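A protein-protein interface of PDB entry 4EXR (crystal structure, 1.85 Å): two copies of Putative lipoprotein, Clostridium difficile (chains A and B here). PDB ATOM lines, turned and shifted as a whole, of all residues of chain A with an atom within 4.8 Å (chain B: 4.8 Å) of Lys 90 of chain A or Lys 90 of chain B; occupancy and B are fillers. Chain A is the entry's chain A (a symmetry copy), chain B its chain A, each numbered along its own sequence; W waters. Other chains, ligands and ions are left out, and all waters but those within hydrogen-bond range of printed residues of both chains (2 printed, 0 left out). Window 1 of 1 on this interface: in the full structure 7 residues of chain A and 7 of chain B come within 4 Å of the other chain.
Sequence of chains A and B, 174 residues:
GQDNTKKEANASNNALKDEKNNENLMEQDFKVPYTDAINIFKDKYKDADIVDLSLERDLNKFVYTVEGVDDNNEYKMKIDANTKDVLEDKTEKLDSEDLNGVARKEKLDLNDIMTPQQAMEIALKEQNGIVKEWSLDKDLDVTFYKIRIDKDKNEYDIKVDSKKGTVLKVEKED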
ATOM      1  N   GLU A  74     -13.665 -18.517  -4.690  1.00  0.00           N
ATOM      2  CA  GLU A  74     -13.626 -19.961  -4.520  1.00  0.00           C
ATOM      3  C   GLU A  74     -15.046 -20.464  -4.340  1.00  0.00           C
ATOM      4  O   GLU A  74     -15.905 -19.765  -3.789  1.00  0.00           O
ATOM      5  CB  GLU A  74     -12.764 -20.379  -3.330  1.00  0.00           C
ATOM      6  CG  GLU A  74     -13.031 -19.631  -2.050  1.00  0.00           C
ATOM      7  CD  GLU A  74     -12.039 -20.012  -0.968  1.00  0.00           C
ATOM      8  OE1 GLU A  74     -11.598 -21.181  -0.965  1.00  0.00           O
ATOM      9  OE2 GLU A  74     -11.692 -19.145  -0.136  1.00  0.00           O
ATOM     10  N   TYR A  75     -15.281 -21.679  -4.814  1.00  0.00           N
ATOM     11  CA  TYR A  75     -16.618 -22.262  -4.812  1.00  0.00           C
ATOM     12  C   TYR A  75     -16.505 -23.640  -4.198  1.00  0.00           C
ATOM     13  O   TYR A  75     -15.542 -24.364  -4.456  1.00  0.00           O
ATOM     14  CB  TYR A  75     -17.135 -22.421  -6.234  1.00  0.00           C
ATOM     15  CG  TYR A  75     -17.208 -21.144  -7.013  1.00  0.00           C
ATOM     16  CD1 TYR A  75     -18.245 -20.242  -6.804  1.00  0.00           C
ATOM     17  CD2 TYR A  75     -16.241 -20.829  -7.967  1.00  0.00           C
ATOM     18  CE1 TYR A  75     -18.313 -19.053  -7.522  1.00  0.00           C
ATOM     19  CE2 TYR A  75     -16.313 -19.659  -8.690  1.00  0.00           C
ATOM     20  CZ  TYR A  75     -17.349 -18.775  -8.464  1.00  0.00           C
ATOM     21  OH  TYR A  75     -17.415 -17.603  -9.183  1.00  0.00           O
ATOM     22  N   LYS A  76     -17.484 -24.004  -3.378  1.00  0.00           N
ATOM     23  CA  LYS A  76     -17.486 -25.322  -2.771  1.00  0.00           C
ATOM     24  C   LYS A  76     -18.886 -25.892  -2.800  1.00  0.00           C
ATOM     25  O   LYS A  76     -19.853 -25.240  -2.394  1.00  0.00           O
ATOM     26  CB  LYS A  76     -16.955 -25.291  -1.340  1.00  0.00           C
ATOM     27  CG  LYS A  76     -16.980 -26.667  -0.675  1.00  0.00           C
ATOM     28  CD  LYS A  76     -16.284 -26.677   0.671  1.00  0.00           C
ATOM     29  CE  LYS A  76     -17.048 -25.872   1.697  1.00  0.00           C
ATOM     30  NZ  LYS A  76     -16.452 -26.037   3.053  1.00  0.00           N
ATOM     31  N   GLU A  88     -24.593 -28.356   0.155  1.00  0.00           N
ATOM     32  CA  GLU A  88     -23.981 -27.052   0.373  1.00  0.00           C
ATOM     33  C   GLU A  88     -23.559 -26.471  -0.963  1.00  0.00           C
ATOM     34  O   GLU A  88     -23.112 -27.198  -1.844  1.00  0.00           O
ATOM     35  CB  GLU A  88     -22.782 -27.137   1.322  1.00  0.00           C
ATOM     36  CG  GLU A  88     -22.148 -25.764   1.588  1.00  0.00           C
ATOM     37  CD  GLU A  88     -20.948 -25.794   2.522  1.00  0.00           C
ATOM     38  OE1 GLU A  88     -20.468 -26.888   2.874  1.00  0.00           O
ATOM     39  OE2 GLU A  88     -20.476 -24.701   2.900  1.00  0.00           O
ATOM     40  N   ASP A  89     -23.717 -25.158  -1.114  1.00  0.00           N
ATOM     41  CA  ASP A  89     -23.227 -24.453  -2.291  1.00  0.00           C
ATOM     42  C   ASP A  89     -22.713 -23.108  -1.781  1.00  0.00           C
ATOM     43  O   ASP A  89     -23.501 -22.238  -1.405  1.00  0.00           O
ATOM     44  CB  ASP A  89     -24.367 -24.272  -3.299  1.00  0.00           C
ATOM     45  CG  ASP A  89     -23.923 -23.605  -4.594  1.00  0.00           C
ATOM     46  OD1 ASP A  89     -22.805 -23.040  -4.655  1.00  0.00           O
ATOM     47  OD2 ASP A  89     -24.717 -23.623  -5.558  1.00  0.00           O
ATOM     48  N   LYS A  90     -21.393 -22.959  -1.747  1.00  0.00           N
ATOM     49  CA  LYS A  90     -20.783 -21.810  -1.094  1.00  0.00           C
ATOM     50  C   LYS A  90     -19.829 -21.089  -2.040  1.00  0.00           C
ATOM     51  O   LYS A  90     -18.973 -21.718  -2.664  1.00  0.00           O
ATOM     52  CB  LYS A  90     -20.032 -22.281   0.151  1.00  0.00           C
ATOM     53  CG  LYS A  90     -19.366 -21.182   0.956  1.00  0.00           C
ATOM     54  CD  LYS A  90     -18.482 -21.811   2.008  1.00  0.00           C
ATOM     55  CE  LYS A  90     -17.980 -20.809   3.014  1.00  0.00           C
ATOM     56  NZ  LYS A  90     -16.919 -21.422   3.865  1.00  0.00           N
ATOM     57  N   THR A  91     -20.006 -19.775  -2.151  1.00  0.00           N
ATOM     58  CA  THR A  91     -19.093 -18.911  -2.890  1.00  0.00           C
ATOM     59  C   THR A  91     -18.442 -17.974  -1.874  1.00  0.00           C
ATOM     60  O   THR A  91     -19.133 -17.436  -1.014  1.00  0.00           O
ATOM     61  CB  THR A  91     -19.870 -18.028  -3.890  1.00  0.00           C
ATOM     62  OG1 THR A  91     -20.621 -18.859  -4.787  1.00  0.00           O
ATOM     63  CG2 THR A  91     -18.912 -17.130  -4.692  1.00  0.00           C
ATOM     64  N   GLU A  92     -17.129 -17.771  -1.974  1.00  0.00           N
ATOM     65  CA  GLU A  92     -16.436 -16.780  -1.148  1.00  0.00           C
ATOM     66  C   GLU A  92     -15.424 -16.042  -2.004  1.00  0.00           C
ATOM     67  O   GLU A  92     -14.738 -16.656  -2.821  1.00  0.00           O
ATOM     68  CB  GLU A  92     -15.647 -17.449  -0.018  1.00  0.00           C
ATOM     69  CG  GLU A  92     -16.399 -17.796   1.242  1.00  0.00           C
ATOM     70  CD  GLU A  92     -15.460 -18.329   2.318  1.00  0.00           C
ATOM     71  OE1 GLU A  92     -15.114 -19.528   2.267  1.00  0.00           O
ATOM     72  OE2 GLU A  92     -15.045 -17.542   3.198  1.00  0.00           O
ATOM     73  N   GLU B  74     -30.962 -22.925   4.238  1.00  0.00           N
ATOM     74  CA  GLU B  74     -30.574 -21.646   4.812  1.00  0.00           C
ATOM     75  C   GLU B  74     -29.588 -20.975   3.874  1.00  0.00           C
ATOM     76  O   GLU B  74     -28.808 -21.644   3.185  1.00  0.00           O
ATOM     77  CB  GLU B  74     -29.958 -21.800   6.202  1.00  0.00           C
ATOM     78  CG  GLU B  74     -28.892 -22.858   6.318  1.00  0.00           C
ATOM     79  CD  GLU B  74     -28.441 -23.035   7.755  1.00  0.00           C
ATOM     80  OE1 GLU B  74     -28.454 -22.031   8.500  1.00  0.00           O
ATOM     81  OE2 GLU B  74     -28.090 -24.172   8.142  1.00  0.00           O
ATOM     82  N   TYR B  75     -29.635 -19.651   3.855  1.00  0.00           N
ATOM     83  CA  TYR B  75     -28.826 -18.864   2.933  1.00  0.00           C
ATOM     84  C   TYR B  75     -28.120 -17.802   3.748  1.00  0.00           C
ATOM     85  O   TYR B  75     -28.705 -17.225   4.665  1.00  0.00           O
ATOM     86  CB  TYR B  75     -29.708 -18.163   1.910  1.00  0.00           C
ATOM     87  CG  TYR B  75     -30.553 -19.085   1.086  1.00  0.00           C
ATOM     88  CD1 TYR B  75     -30.003 -19.798   0.027  1.00  0.00           C
ATOM     89  CD2 TYR B  75     -31.912 -19.248   1.357  1.00  0.00           C
ATOM     90  CE1 TYR B  75     -30.784 -20.659  -0.736  1.00  0.00           C
ATOM     91  CE2 TYR B  75     -32.691 -20.089   0.594  1.00  0.00           C
ATOM     92  CZ  TYR B  75     -32.123 -20.791  -0.450  1.00  0.00           C
ATOM     93  OH  TYR B  75     -32.903 -21.636  -1.207  1.00  0.00           O
ATOM     94  N   LYS B  76     -26.858 -17.548   3.422  1.00  0.00           N
ATOM     95  CA  LYS B  76     -26.110 -16.519   4.119  1.00  0.00           C
ATOM     96  C   LYS B  76     -25.295 -15.723   3.124  1.00  0.00           C
ATOM     97  O   LYS B  76     -24.571 -16.280   2.294  1.00  0.00           O
ATOM     98  CB  LYS B  76     -25.203 -17.107   5.198  1.00  0.00           C
ATOM     99  CG  LYS B  76     -24.383 -16.038   5.920  1.00  0.00           C
ATOM    100  CD  LYS B  76     -23.626 -16.591   7.111  1.00  0.00           C
ATOM    101  CE  LYS B  76     -22.521 -17.527   6.681  1.00  0.00           C
ATOM    102  NZ  LYS B  76     -21.675 -17.921   7.843  1.00  0.00           N
ATOM    103  N   GLU B  88     -19.394 -13.333   0.508  1.00  0.00           N
ATOM    104  CA  GLU B  88     -19.774 -14.727   0.695  1.00  0.00           C
ATOM    105  C   GLU B  88     -21.214 -14.914   0.255  1.00  0.00           C
ATOM    106  O   GLU B  88     -22.047 -14.038   0.463  1.00  0.00           O
ATOM    107  CB  GLU B  88     -19.597 -15.175   2.149  1.00  0.00           C
ATOM    108  CG  GLU B  88     -19.961 -16.652   2.355  1.00  0.00           C
ATOM    109  CD  GLU B  88     -19.807 -17.146   3.785  1.00  0.00           C
ATOM    110  OE1 GLU B  88     -19.564 -16.332   4.696  1.00  0.00           O
ATOM    111  OE2 GLU B  88     -19.941 -18.370   3.997  1.00  0.00           O
ATOM    112  N   ASP B  89     -21.498 -16.056  -0.367  1.00  0.00           N
ATOM    113  CA  ASP B  89     -22.864 -16.422  -0.719  1.00  0.00           C
ATOM    114  C   ASP B  89     -22.957 -17.930  -0.493  1.00  0.00           C
ATOM    115  O   ASP B  89     -22.392 -18.714  -1.259  1.00  0.00           O
ATOM    116  CB  ASP B  89     -23.139 -16.056  -2.181  1.00  0.00           C
ATOM    117  CG  ASP B  89     -24.572 -16.340  -2.612  1.00  0.00           C
ATOM    118  OD1 ASP B  89     -25.311 -17.051  -1.892  1.00  0.00           O
ATOM    119  OD2 ASP B  89     -24.953 -15.866  -3.703  1.00  0.00           O
ATOM    120  N   LYS B  90     -23.647 -18.323   0.572  1.00  0.00           N
ATOM    121  CA  LYS B  90     -23.636 -19.712   1.005  1.00  0.00           C
ATOM    122  C   LYS B  90     -25.055 -20.253   1.138  1.00  0.00           C
ATOM    123  O   LYS B  90     -25.907 -19.627   1.770  1.00  0.00           O
ATOM    124  CB  LYS B  90     -22.907 -19.814   2.344  1.00  0.00           C
ATOM    125  CG  LYS B  90     -22.788 -21.217   2.908  1.00  0.00           C
ATOM    126  CD  LYS B  90     -22.260 -21.135   4.322  1.00  0.00           C
ATOM    127  CE  LYS B  90     -21.871 -22.481   4.871  1.00  0.00           C
ATOM    128  NZ  LYS B  90     -21.606 -22.382   6.336  1.00  0.00           N
ATOM    129  N   THR B  91     -25.297 -21.406   0.518  1.00  0.00           N
ATOM    130  CA  THR B  91     -26.549 -22.139   0.665  1.00  0.00           C
ATOM    131  C   THR B  91     -26.218 -23.456   1.364  1.00  0.00           C
ATOM    132  O   THR B  91     -25.239 -24.104   1.005  1.00  0.00           O
ATOM    133  CB  THR B  91     -27.136 -22.493  -0.719  1.00  0.00           C
ATOM    134  OG1 THR B  91     -27.336 -21.295  -1.481  1.00  0.00           O
ATOM    135  CG2 THR B  91     -28.471 -23.246  -0.573  1.00  0.00           C
ATOM    136  N   GLU B  92     -27.025 -23.853   2.345  1.00  0.00           N
ATOM    137  CA  GLU B  92     -26.884 -25.168   2.976  1.00  0.00           C
ATOM    138  C   GLU B  92     -28.262 -25.764   3.193  1.00  0.00           C
ATOM    139  O   GLU B  92     -29.188 -25.058   3.592  1.00  0.00           O
ATOM    140  CB  GLU B  92     -26.234 -25.056   4.358  1.00  0.00           C
ATOM    141  CG  GLU B  92     -24.728 -25.000   4.415  1.00  0.00           C
ATOM    142  CD  GLU B  92     -24.227 -25.026   5.855  1.00  0.00           C
ATOM    143  OE1 GLU B  92     -24.229 -23.959   6.506  1.00  0.00           O
ATOM    144  OE2 GLU B  92     -23.858 -26.116   6.344  1.00  0.00           O
HETATM  145  O   HOH W   1     -25.126 -19.968  -2.524  1.00  0.00           O
HETATM  146  O   HOH W   2     -22.890 -20.162  -3.847  1.00  0.00           O
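Of chain B, only Glu 88, Asp 89 and Lys 90 come within 4 Å of Lys 90 of chain A. Of chain A, only Glu 88, Asp 89 and Lys 90 come within 4 Å of Lys 90 of chain B. Of the printed residues of chain A, Glu 92 of chain B touches Glu 88 (3.9 Å). Of the printed residues of chain A, Glu 88 of chain B touches Lys 90 (3.3 Å), Thr 91 (3.3 Å) and Glu 92 (3.9 Å). Of the printed residues of chain B, Thr 91 of chain A touches Glu 88 (3.3 Å) and Asp 89 (2.8 Å). Printed residues of chain B within 4 Å of Asp 89 of chain A: Asp 89, Lys 90 and Thr 91. Of the printed residues of chain A, Asp 89 of chain B touches Asp 89, Lys 90 and Thr 91. Lys 76 of chain A touches none of the printed residues of chain B. Tyr 75 of chain A touches none of the printed residues of chain B.
Printed residues of chain A that touch a printed residue of chain B: Glu 88, Asp 89, Lys 90, Thr 91 and Glu 92. Among the printed residues, no Asp or Glu carboxylate lies within 4 Å of a Lys or Arg side-chain nitrogen of the other chain.
The backbone carbonyl oxygen of Asp 89 of chain A is in hydrogen-bond range of the backbone NH of Thr 91 of chain B (2.8 Å). N of Thr 91 of chain A lies within hydrogen-bond range of O of Asp 89 of chain B (2.8 Å).
N of Glu 74 of chain A lies within hydrogen-bond range of O of Glu 92 of chain A, at 2.8 Å. OE1 of Glu 92 of chain A is in salt-bridge range of NZ of Lys 90 of chain A, 3.1 Å away. O of Glu 92 of chain B lies within hydrogen-bond range of N of Glu 74 of chain B. The backbone NH (N) of Lys 76 of chain A is in hydrogen-bond range of the backbone carbonyl oxygen (O) of Lys 90 of chain A. N of Lys 76 of chain B lies within hydrogen-bond range of O of Lys 90 of chain B (2.8 Å). The side-chain carboxylate (OE1) of Glu 92 of chain B is in salt-bridge range of the side-chain amino group (NZ) of Lys 90 of chain B.
Water W1 lies within hydrogen-bond range of OG1 of Thr 91 of chain B, OD1 of Asp 89 of chain B and O of Asp 89 of chain A. Water W2 lies within hydrogen-bond range of the side-chain hydroxyl of Thr 91 of chain A (2.8 Å), the side-chain carboxylate of Asp 89 of chain A (3.0 Å) and the backbone carbonyl oxygen of Asp 89 of chain B (3.0 Å).
Glu 88 of chain A touches Lys 90 of chain B, and with the chains exchanged Lys 90 of chain A touches Glu 88 of chain B. Glu 88 of chain A touches Thr 91 of chain B, and with the chains exchanged Thr 91 of chain A touches Glu 88 of chain B. Asp 89 of chain A touches Lys 90 of chain B, and with the chains exchanged Lys 90 of chain A touches Asp 89 of chain B. Asp 89 of chain A touches Thr 91 of chain B, and with the chains exchanged Thr 91 of chain A touches Asp 89 of chain B. Of the 12 pairs that touch across the chains among the printed residues, 12 have their exchanged pair printed and touching as well.
Among the printed residues, merely in contact across the chains: Thr 91 of chain A with Glu 88 of chain B (3.3 Å), Glu 88 of chain A with Thr 91 of chain B (3.3 Å), Glu 88 of chain A with Lys 90 of chain B (3.3 Å), Lys 90 of chain A with Glu 88 of chain B (3.3 Å), Lys 90 of chain A with Asp 89 of chain B (3.5 Å), Asp 89 of chain A with Lys 90 of chain B (3.5 Å), Asp 89 of chain A with Asp 89 of chain B (3.7 Å), Glu 88 of chain A with Glu 92 of chain B (3.9 Å), Glu 92 of chain A with Glu 88 of chain B (3.9 Å) and Lys 90 of chain A with Lys 90 of chain B (3.9 Å).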
